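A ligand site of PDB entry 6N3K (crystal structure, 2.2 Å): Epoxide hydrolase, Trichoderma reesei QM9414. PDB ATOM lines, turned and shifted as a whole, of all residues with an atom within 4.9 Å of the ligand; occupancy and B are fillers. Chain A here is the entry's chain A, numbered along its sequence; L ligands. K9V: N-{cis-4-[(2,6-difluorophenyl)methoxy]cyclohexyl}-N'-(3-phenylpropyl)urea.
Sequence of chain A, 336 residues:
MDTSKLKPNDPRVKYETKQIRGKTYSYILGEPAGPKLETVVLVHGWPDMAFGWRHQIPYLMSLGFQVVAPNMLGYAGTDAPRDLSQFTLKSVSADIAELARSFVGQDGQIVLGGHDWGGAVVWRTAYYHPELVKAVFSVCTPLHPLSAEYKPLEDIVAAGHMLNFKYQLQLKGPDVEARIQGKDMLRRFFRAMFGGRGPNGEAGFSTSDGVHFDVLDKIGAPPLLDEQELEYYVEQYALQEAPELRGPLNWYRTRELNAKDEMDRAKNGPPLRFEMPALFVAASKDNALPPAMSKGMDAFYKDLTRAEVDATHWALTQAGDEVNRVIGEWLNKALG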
ATOM      1  N   TRP A  46      19.625  -1.363 -11.465  1.00  0.00           N
ATOM      2  CA  TRP A  46      19.739  -0.822 -10.105  1.00  0.00           C
ATOM      3  C   TRP A  46      18.408  -0.855  -9.367  1.00  0.00           C
ATOM      4  O   TRP A  46      17.395  -0.475  -9.926  1.00  0.00           O
ATOM      5  CB  TRP A  46      20.258   0.617 -10.130  1.00  0.00           C
ATOM      6  CG  TRP A  46      20.632   1.168  -8.768  1.00  0.00           C
ATOM      7  CD1 TRP A  46      21.866   1.139  -8.185  1.00  0.00           C
ATOM      8  CD2 TRP A  46      19.764   1.834  -7.835  1.00  0.00           C
ATOM      9  NE1 TRP A  46      21.822   1.741  -6.946  1.00  0.00           N
ATOM     10  CE2 TRP A  46      20.532   2.167  -6.699  1.00  0.00           C
ATOM     11  CE3 TRP A  46      18.405   2.174  -7.837  1.00  0.00           C
ATOM     12  CZ2 TRP A  46      19.999   2.843  -5.595  1.00  0.00           C
ATOM     13  CZ3 TRP A  46      17.863   2.830  -6.725  1.00  0.00           C
ATOM     14  CH2 TRP A  46      18.671   3.155  -5.626  1.00  0.00           C
ATOM     15  N   PRO A  47      18.421  -1.269  -8.085  1.00  0.00           N
ATOM     16  CA  PRO A  47      19.509  -1.890  -7.324  1.00  0.00           C
ATOM     17  C   PRO A  47      19.287  -3.393  -7.291  1.00  0.00           C
ATOM     18  O   PRO A  47      18.688  -3.918  -6.339  1.00  0.00           O
ATOM     19  CB  PRO A  47      19.345  -1.276  -5.930  1.00  0.00           C
ATOM     20  CG  PRO A  47      17.852  -1.084  -5.797  1.00  0.00           C
ATOM     21  CD  PRO A  47      17.282  -0.951  -7.197  1.00  0.00           C
ATOM     22  N   ASP A 116      16.450  -2.310 -16.925  1.00  0.00           N
ATOM     23  CA  ASP A 116      16.796  -1.092 -16.165  1.00  0.00           C
ATOM     24  C   ASP A 116      18.099  -0.538 -16.729  1.00  0.00           C
ATOM     25  O   ASP A 116      18.195  -0.369 -17.963  1.00  0.00           O
ATOM     26  CB  ASP A 116      16.814  -1.403 -14.679  1.00  0.00           C
ATOM     27  CG  ASP A 116      17.155  -0.180 -13.841  1.00  0.00           C
ATOM     28  OD1 ASP A 116      16.265   0.680 -13.736  1.00  0.00           O
ATOM     29  OD2 ASP A 116      18.285  -0.062 -13.317  1.00  0.00           O
ATOM     30  N   TRP A 117      19.111  -0.248 -15.902  1.00  0.00           N
ATOM     31  CA  TRP A 117      20.398   0.172 -16.410  1.00  0.00           C
ATOM     32  C   TRP A 117      20.963  -0.853 -17.377  1.00  0.00           C
ATOM     33  O   TRP A 117      21.641  -0.492 -18.350  1.00  0.00           O
ATOM     34  CB  TRP A 117      21.371   0.404 -15.258  1.00  0.00           C
ATOM     35  CG  TRP A 117      21.424   1.829 -14.810  1.00  0.00           C
ATOM     36  CD1 TRP A 117      21.123   2.325 -13.570  1.00  0.00           C
ATOM     37  CD2 TRP A 117      21.797   2.971 -15.609  1.00  0.00           C
ATOM     38  NE1 TRP A 117      21.286   3.680 -13.545  1.00  0.00           N
ATOM     39  CE2 TRP A 117      21.691   4.109 -14.782  1.00  0.00           C
ATOM     40  CE3 TRP A 117      22.197   3.136 -16.932  1.00  0.00           C
ATOM     41  CZ2 TRP A 117      21.991   5.396 -15.241  1.00  0.00           C
ATOM     42  CZ3 TRP A 117      22.484   4.408 -17.391  1.00  0.00           C
ATOM     43  CH2 TRP A 117      22.374   5.524 -16.548  1.00  0.00           C
ATOM     44  N   ALA A 120      19.768  -0.216 -20.857  1.00  0.00           N
ATOM     45  CA  ALA A 120      20.571   0.823 -21.504  1.00  0.00           C
ATOM     46  C   ALA A 120      21.892   0.262 -21.990  1.00  0.00           C
ATOM     47  O   ALA A 120      22.361   0.594 -23.087  1.00  0.00           O
ATOM     48  CB  ALA A 120      20.796   1.988 -20.545  1.00  0.00           C
ATOM     49  N   THR A 141      13.544  -0.819 -20.310  1.00  0.00           N
ATOM     50  CA  THR A 141      14.365   0.325 -20.744  1.00  0.00           C
ATOM     51  C   THR A 141      14.294   0.496 -22.257  1.00  0.00           C
ATOM     52  O   THR A 141      14.753  -0.396 -22.994  1.00  0.00           O
ATOM     53  CB  THR A 141      15.818   0.142 -20.338  1.00  0.00           C
ATOM     54  OG1 THR A 141      15.888  -0.228 -18.967  1.00  0.00           O
ATOM     55  CG2 THR A 141      16.598   1.430 -20.535  1.00  0.00           C
ATOM     56  N   PRO A 142      13.761   1.600 -22.765  1.00  0.00           N
ATOM     57  CA  PRO A 142      13.781   1.837 -24.209  1.00  0.00           C
ATOM     58  C   PRO A 142      15.113   2.445 -24.639  1.00  0.00           C
ATOM     59  O   PRO A 142      15.946   2.814 -23.815  1.00  0.00           O
ATOM     60  CB  PRO A 142      12.630   2.822 -24.409  1.00  0.00           C
ATOM     61  CG  PRO A 142      12.676   3.638 -23.190  1.00  0.00           C
ATOM     62  CD  PRO A 142      13.112   2.714 -22.055  1.00  0.00           C
ATOM     63  N   HIS A 144      17.631   5.198 -25.814  1.00  0.00           N
ATOM     64  CA  HIS A 144      17.713   6.638 -25.851  1.00  0.00           C
ATOM     65  C   HIS A 144      18.761   7.044 -26.890  1.00  0.00           C
ATOM     66  O   HIS A 144      19.697   6.291 -27.152  1.00  0.00           O
ATOM     67  CB  HIS A 144      18.049   7.249 -24.479  1.00  0.00           C
ATOM     68  CG  HIS A 144      19.455   6.987 -23.998  1.00  0.00           C
ATOM     69  ND1 HIS A 144      19.890   5.743 -23.602  1.00  0.00           N
ATOM     70  CD2 HIS A 144      20.497   7.827 -23.810  1.00  0.00           C
ATOM     71  CE1 HIS A 144      21.145   5.817 -23.214  1.00  0.00           C
ATOM     72  NE2 HIS A 144      21.539   7.073 -23.320  1.00  0.00           N
ATOM     73  N   MET A 162      12.168  15.674 -17.656  1.00  0.00           N
ATOM     74  CA  MET A 162      12.679  14.402 -17.154  1.00  0.00           C
ATOM     75  C   MET A 162      12.387  14.260 -15.669  1.00  0.00           C
ATOM     76  O   MET A 162      13.211  13.767 -14.891  1.00  0.00           O
ATOM     77  CB  MET A 162      14.180  14.284 -17.416  1.00  0.00           C
ATOM     78  CG  MET A 162      14.576  14.105 -18.888  1.00  0.00           C
ATOM     79  SD  MET A 162      16.356  13.818 -19.095  1.00  0.00           S
ATOM     80  CE  MET A 162      16.398  13.005 -20.691  1.00  0.00           C
ATOM     81  N   PHE A 165      13.016  11.222 -13.610  1.00  0.00           N
ATOM     82  CA  PHE A 165      14.410  10.877 -13.323  1.00  0.00           C
ATOM     83  C   PHE A 165      15.013  11.665 -12.166  1.00  0.00           C
ATOM     84  O   PHE A 165      16.203  11.503 -11.867  1.00  0.00           O
ATOM     85  CB  PHE A 165      15.275  11.097 -14.572  1.00  0.00           C
ATOM     86  CG  PHE A 165      15.118  10.046 -15.635  1.00  0.00           C
ATOM     87  CD1 PHE A 165      14.995   8.709 -15.306  1.00  0.00           C
ATOM     88  CD2 PHE A 165      15.102  10.395 -16.982  1.00  0.00           C
ATOM     89  CE1 PHE A 165      14.859   7.719 -16.302  1.00  0.00           C
ATOM     90  CE2 PHE A 165      14.981   9.431 -17.986  1.00  0.00           C
ATOM     91  CZ  PHE A 165      14.860   8.079 -17.640  1.00  0.00           C
ATOM     92  N   TYR A 167      14.885  11.511  -9.045  1.00  0.00           N
ATOM     93  CA  TYR A 167      15.452  10.670  -7.988  1.00  0.00           C
ATOM     94  C   TYR A 167      16.942  10.428  -8.181  1.00  0.00           C
ATOM     95  O   TYR A 167      17.643  10.138  -7.205  1.00  0.00           O
ATOM     96  CB  TYR A 167      14.727   9.320  -7.935  1.00  0.00           C
ATOM     97  CG  TYR A 167      15.057   8.411  -9.103  1.00  0.00           C
ATOM     98  CD1 TYR A 167      14.312   8.472 -10.273  1.00  0.00           C
ATOM     99  CD2 TYR A 167      16.106   7.504  -9.033  1.00  0.00           C
ATOM    100  CE1 TYR A 167      14.608   7.646 -11.348  1.00  0.00           C
ATOM    101  CE2 TYR A 167      16.430   6.679 -10.096  1.00  0.00           C
ATOM    102  CZ  TYR A 167      15.673   6.752 -11.255  1.00  0.00           C
ATOM    103  OH  TYR A 167      15.990   5.920 -12.318  1.00  0.00           O
ATOM    104  N   GLN A 168      17.435  10.511  -9.433  1.00  0.00           N
ATOM    105  CA  GLN A 168      18.837  10.227  -9.696  1.00  0.00           C
ATOM    106  C   GLN A 168      19.758  11.308  -9.134  1.00  0.00           C
ATOM    107  O   GLN A 168      20.965  11.050  -8.988  1.00  0.00           O
ATOM    108  CB  GLN A 168      19.084  10.087 -11.205  1.00  0.00           C
ATOM    109  CG  GLN A 168      18.382   8.905 -11.857  1.00  0.00           C
ATOM    110  CD  GLN A 168      18.689   8.806 -13.341  1.00  0.00           C
ATOM    111  OE1 GLN A 168      19.498   9.545 -13.875  1.00  0.00           O
ATOM    112  NE2 GLN A 168      18.028   7.881 -14.017  1.00  0.00           N
ATOM    113  N   MET A 193      12.907  -0.603  -1.724  1.00  0.00           N
ATOM    114  CA  MET A 193      13.066  -0.624  -3.179  1.00  0.00           C
ATOM    115  C   MET A 193      12.138  -1.619  -3.844  1.00  0.00           C
ATOM    116  O   MET A 193      11.775  -1.442  -5.015  1.00  0.00           O
ATOM    117  CB  MET A 193      14.504  -0.928  -3.557  1.00  0.00           C
ATOM    118  CG  MET A 193      15.481   0.184  -3.157  1.00  0.00           C
ATOM    119  SD  MET A 193      15.011   1.808  -3.809  1.00  0.00           S
ATOM    120  CE  MET A 193      14.843   1.476  -5.557  1.00  0.00           C
ATOM    121  N   PHE A 205      10.663   4.783  -1.340  1.00  0.00           N
ATOM    122  CA  PHE A 205      11.359   5.249  -2.531  1.00  0.00           C
ATOM    123  C   PHE A 205      10.321   5.852  -3.463  1.00  0.00           C
ATOM    124  O   PHE A 205       9.217   5.323  -3.593  1.00  0.00           O
ATOM    125  CB  PHE A 205      12.114   4.121  -3.255  1.00  0.00           C
ATOM    126  CG  PHE A 205      12.735   4.559  -4.566  1.00  0.00           C
ATOM    127  CD1 PHE A 205      12.016   4.517  -5.750  1.00  0.00           C
ATOM    128  CD2 PHE A 205      14.029   5.067  -4.596  1.00  0.00           C
ATOM    129  CE1 PHE A 205      12.565   4.952  -6.928  1.00  0.00           C
ATOM    130  CE2 PHE A 205      14.598   5.498  -5.784  1.00  0.00           C
ATOM    131  CZ  PHE A 205      13.867   5.426  -6.952  1.00  0.00           C
ATOM    132  N   THR A 207      10.131   8.165  -7.456  1.00  0.00           N
ATOM    133  CA  THR A 207      10.932   8.671  -8.573  1.00  0.00           C
ATOM    134  C   THR A 207      11.207  10.180  -8.436  1.00  0.00           C
ATOM    135  O   THR A 207      12.110  10.688  -9.103  1.00  0.00           O
ATOM    136  CB  THR A 207      10.254   8.365  -9.916  1.00  0.00           C
ATOM    137  OG1 THR A 207       8.922   8.881  -9.935  1.00  0.00           O
ATOM    138  CG2 THR A 207      10.194   6.837 -10.189  1.00  0.00           C
ATOM    139  N   TYR A 252      24.971   6.423 -11.443  1.00  0.00           N
ATOM    140  CA  TYR A 252      24.263   7.683 -11.589  1.00  0.00           C
ATOM    141  C   TYR A 252      25.211   8.874 -11.639  1.00  0.00           C
ATOM    142  O   TYR A 252      24.755  10.017 -11.618  1.00  0.00           O
ATOM    143  CB  TYR A 252      23.239   7.832 -10.473  1.00  0.00           C
ATOM    144  CG  TYR A 252      22.232   6.720 -10.526  1.00  0.00           C
ATOM    145  CD1 TYR A 252      21.100   6.832 -11.320  1.00  0.00           C
ATOM    146  CD2 TYR A 252      22.426   5.543  -9.823  1.00  0.00           C
ATOM    147  CE1 TYR A 252      20.168   5.813 -11.381  1.00  0.00           C
ATOM    148  CE2 TYR A 252      21.511   4.523  -9.881  1.00  0.00           C
ATOM    149  CZ  TYR A 252      20.384   4.656 -10.656  1.00  0.00           C
ATOM    150  OH  TYR A 252      19.477   3.644 -10.715  1.00  0.00           O
ATOM    151  N   ASP A 286       5.650   0.735 -14.660  1.00  0.00           N
ATOM    152  CA  ASP A 286       6.986   1.259 -14.384  1.00  0.00           C
ATOM    153  C   ASP A 286       6.877   2.775 -14.469  1.00  0.00           C
ATOM    154  O   ASP A 286       6.778   3.346 -15.557  1.00  0.00           O
ATOM    155  CB  ASP A 286       8.008   0.710 -15.369  1.00  0.00           C
ATOM    156  CG  ASP A 286       9.440   1.001 -14.947  1.00  0.00           C
ATOM    157  OD1 ASP A 286       9.690   2.037 -14.272  1.00  0.00           O
ATOM    158  OD2 ASP A 286      10.338   0.188 -15.279  1.00  0.00           O
ATOM    159  N   ASN A 287       6.859   3.448 -13.321  1.00  0.00           N
ATOM    160  CA  ASN A 287       6.785   4.907 -13.316  1.00  0.00           C
ATOM    161  C   ASN A 287       8.159   5.571 -13.460  1.00  0.00           C
ATOM    162  O   ASN A 287       8.211   6.783 -13.676  1.00  0.00           O
ATOM    163  CB  ASN A 287       6.072   5.421 -12.058  1.00  0.00           C
ATOM    164  CG  ASN A 287       6.212   4.479 -10.873  1.00  0.00           C
ATOM    165  OD1 ASN A 287       6.877   3.444 -10.966  1.00  0.00           O
ATOM    166  ND2 ASN A 287       5.592   4.844  -9.759  1.00  0.00           N
ATOM    167  N   ALA A 288       9.247   4.816 -13.351  1.00  0.00           N
ATOM    168  CA  ALA A 288      10.555   5.352 -13.705  1.00  0.00           C
ATOM    169  C   ALA A 288      10.785   5.334 -15.208  1.00  0.00           C
ATOM    170  O   ALA A 288      11.404   6.257 -15.750  1.00  0.00           O
ATOM    171  CB  ALA A 288      11.675   4.568 -13.001  1.00  0.00           C
ATOM    172  N   LEU A 289      10.296   4.297 -15.892  1.00  0.00           N
ATOM    173  CA  LEU A 289      10.450   4.133 -17.339  1.00  0.00           C
ATOM    174  C   LEU A 289       9.096   3.786 -17.938  1.00  0.00           C
ATOM    175  O   LEU A 289       8.856   2.647 -18.349  1.00  0.00           O
ATOM    176  CB  LEU A 289      11.486   3.049 -17.651  1.00  0.00           C
ATOM    177  CG  LEU A 289      12.899   3.238 -17.085  1.00  0.00           C
ATOM    178  CD1 LEU A 289      13.679   1.926 -17.124  1.00  0.00           C
ATOM    179  CD2 LEU A 289      13.640   4.332 -17.831  1.00  0.00           C
ATOM    180  N   MET A 293       7.625   6.410 -22.897  1.00  0.00           N
ATOM    181  CA  MET A 293       8.996   6.850 -23.109  1.00  0.00           C
ATOM    182  C   MET A 293       9.636   6.199 -24.332  1.00  0.00           C
ATOM    183  O   MET A 293      10.679   6.677 -24.805  1.00  0.00           O
ATOM    184  CB  MET A 293       9.814   6.536 -21.851  1.00  0.00           C
ATOM    185  CG  MET A 293      11.132   7.250 -21.771  1.00  0.00           C
ATOM    186  SD  MET A 293      11.408   7.794 -20.091  1.00  0.00           S
ATOM    187  CE  MET A 293       9.905   8.731 -19.821  1.00  0.00           C
ATOM    188  N   HIS A 313       8.059  -1.747 -12.338  1.00  0.00           N
ATOM    189  CA  HIS A 313       9.432  -1.804 -12.810  1.00  0.00           C
ATOM    190  C   HIS A 313      10.024  -3.203 -12.656  1.00  0.00           C
ATOM    191  O   HIS A 313      10.860  -3.626 -13.470  1.00  0.00           O
ATOM    192  CB  HIS A 313      10.281  -0.780 -12.065  1.00  0.00           C
ATOM    193  CG  HIS A 313      11.719  -0.761 -12.487  1.00  0.00           C
ATOM    194  ND1 HIS A 313      12.156  -0.133 -13.635  1.00  0.00           N
ATOM    195  CD2 HIS A 313      12.825  -1.305 -11.919  1.00  0.00           C
ATOM    196  CE1 HIS A 313      13.458  -0.288 -13.761  1.00  0.00           C
ATOM    197  NE2 HIS A 313      13.890  -0.995 -12.729  1.00  0.00           N
ATOM    198  N   TRP A 314       9.611  -3.933 -11.629  1.00  0.00           N
ATOM    199  CA  TRP A 314      10.213  -5.233 -11.348  1.00  0.00           C
ATOM    200  C   TRP A 314       9.535  -6.343 -12.162  1.00  0.00           C
ATOM    201  O   TRP A 314       9.029  -7.325 -11.635  1.00  0.00           O
ATOM    202  CB  TRP A 314      10.176  -5.508  -9.851  1.00  0.00           C
ATOM    203  CG  TRP A 314      11.019  -4.545  -9.071  1.00  0.00           C
ATOM    204  CD1 TRP A 314      10.593  -3.711  -8.072  1.00  0.00           C
ATOM    205  CD2 TRP A 314      12.426  -4.298  -9.222  1.00  0.00           C
ATOM    206  NE1 TRP A 314      11.655  -2.969  -7.598  1.00  0.00           N
ATOM    207  CE2 TRP A 314      12.787  -3.308  -8.283  1.00  0.00           C
ATOM    208  CE3 TRP A 314      13.420  -4.822 -10.069  1.00  0.00           C
ATOM    209  CZ2 TRP A 314      14.092  -2.837  -8.164  1.00  0.00           C
ATOM    210  CZ3 TRP A 314      14.717  -4.357  -9.935  1.00  0.00           C
ATOM    211  CH2 TRP A 314      15.042  -3.374  -8.994  1.00  0.00           C
HETATM  212  C10 K9V L   1      10.710   0.993  -7.814  1.00  0.00           C
HETATM  213  C15 K9V L   1      17.706   2.959 -16.672  1.00  0.00           C
HETATM  214  C17 K9V L   1      18.767   4.974 -17.877  1.00  0.00           C
HETATM  215  C20 K9V L   1      17.859   6.949 -20.596  1.00  0.00           C
HETATM  216  C21 K9V L   1      16.774   6.201 -21.037  1.00  0.00           C
HETATM  217  C24 K9V L   1      15.702   8.201 -21.829  1.00  0.00           C
HETATM  218  C26 K9V L   1      17.872   8.330 -20.772  1.00  0.00           C
HETATM  219  C28 K9V L   1      17.711   5.727 -17.048  1.00  0.00           C
HETATM  220  O01 K9V L   1      17.831   3.905 -12.467  1.00  0.00           O
HETATM  221  C02 K9V L   1      17.007   3.233 -12.997  1.00  0.00           C
HETATM  222  N03 K9V L   1      16.054   2.502 -12.175  1.00  0.00           N
HETATM  223  C04 K9V L   1      16.154   2.639 -10.729  1.00  0.00           C
HETATM  224  C05 K9V L   1      14.996   1.890 -10.053  1.00  0.00           C
HETATM  225  C06 K9V L   1      13.654   2.362 -10.578  1.00  0.00           C
HETATM  226  C07 K9V L   1      12.597   1.884  -9.618  1.00  0.00           C
HETATM  227  C08 K9V L   1      12.978   1.008  -8.603  1.00  0.00           C
HETATM  228  C09 K9V L   1      12.032   0.566  -7.698  1.00  0.00           C
HETATM  229  C11 K9V L   1      10.335   1.864  -8.835  1.00  0.00           C
HETATM  230  C12 K9V L   1      11.282   2.319  -9.734  1.00  0.00           C
HETATM  231  N13 K9V L   1      16.919   3.097 -14.449  1.00  0.00           N
HETATM  232  C14 K9V L   1      17.827   3.748 -15.383  1.00  0.00           C
HETATM  233  C16 K9V L   1      18.730   3.453 -17.681  1.00  0.00           C
HETATM  234  O18 K9V L   1      18.465   5.163 -19.234  1.00  0.00           O
HETATM  235  C19 K9V L   1      19.031   6.253 -19.902  1.00  0.00           C
HETATM  236  F22 K9V L   1      16.759   4.849 -20.857  1.00  0.00           F
HETATM  237  C23 K9V L   1      15.696   6.827 -21.653  1.00  0.00           C
HETATM  238  C25 K9V L   1      16.780   8.955 -21.383  1.00  0.00           C
HETATM  239  F27 K9V L   1      18.928   9.076 -20.342  1.00  0.00           F
HETATM  240  C29 K9V L   1      17.476   5.213 -15.622  1.00  0.00           C
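The side-chain carboxylate (OD1) of Asp 116 lies within hydrogen-bond range of a nitrogen (N03) of the ligand, 2.4 Å away.
An oxygen (O01) of the ligand lies within hydrogen-bond range of the side-chain hydroxyl (OH) of Tyr 252, 2.4 Å away.
O01 of the ligand is in hydrogen-bond range of OH of Tyr 167.
The side-chain carboxylate of Asp 116 is in hydrogen-bond range of the backbone NH of Trp 46 (2.6 Å).
The backbone carbonyl oxygen (O) of Asp 116 sits at hydrogen-bond distance from the side-chain hydroxyl (OG1) of Thr 141 (2.5 Å).
The side-chain carboxylate (OD1) of Asp 116 sits close to a ring nitrogen (NE2) of His 313 (3.1 Å).
The side-chain hydroxyl of Tyr 252 lies close to the indole nitrogen of Trp 117, 3.4 Å away.
The side-chain hydroxyl (OH) of Tyr 167 is in hydrogen-bond range of the side-chain amide nitrogen (NE2) of Gln 168 (3.3 Å).
The indole nitrogen of Trp 314 is in hydrogen-bond range of the backbone carbonyl oxygen of Met 193 (3.0 Å).
OD1 of Asp 286 is in hydrogen-bond range of N of Ala 288 (3.0 Å).
ND1 of His 313 lies within hydrogen-bond range of OD2 of Asp 286 (2.5 Å).
Merely in contact with the ligand: Trp 46, Trp 117, Ala 120, Thr 141, Pro 142, His 144, Phe 165, Gln 168, Met 193, Ala 288, His 313 and Trp 314.
Hydrophobic or aromatic side chains within 4 Å of the ligand: Trp 46, Trp 117, Ala 120, His 144, Phe 165, Tyr 167, Met 193, Tyr 252, Ala 288, His 313 and Trp 314.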
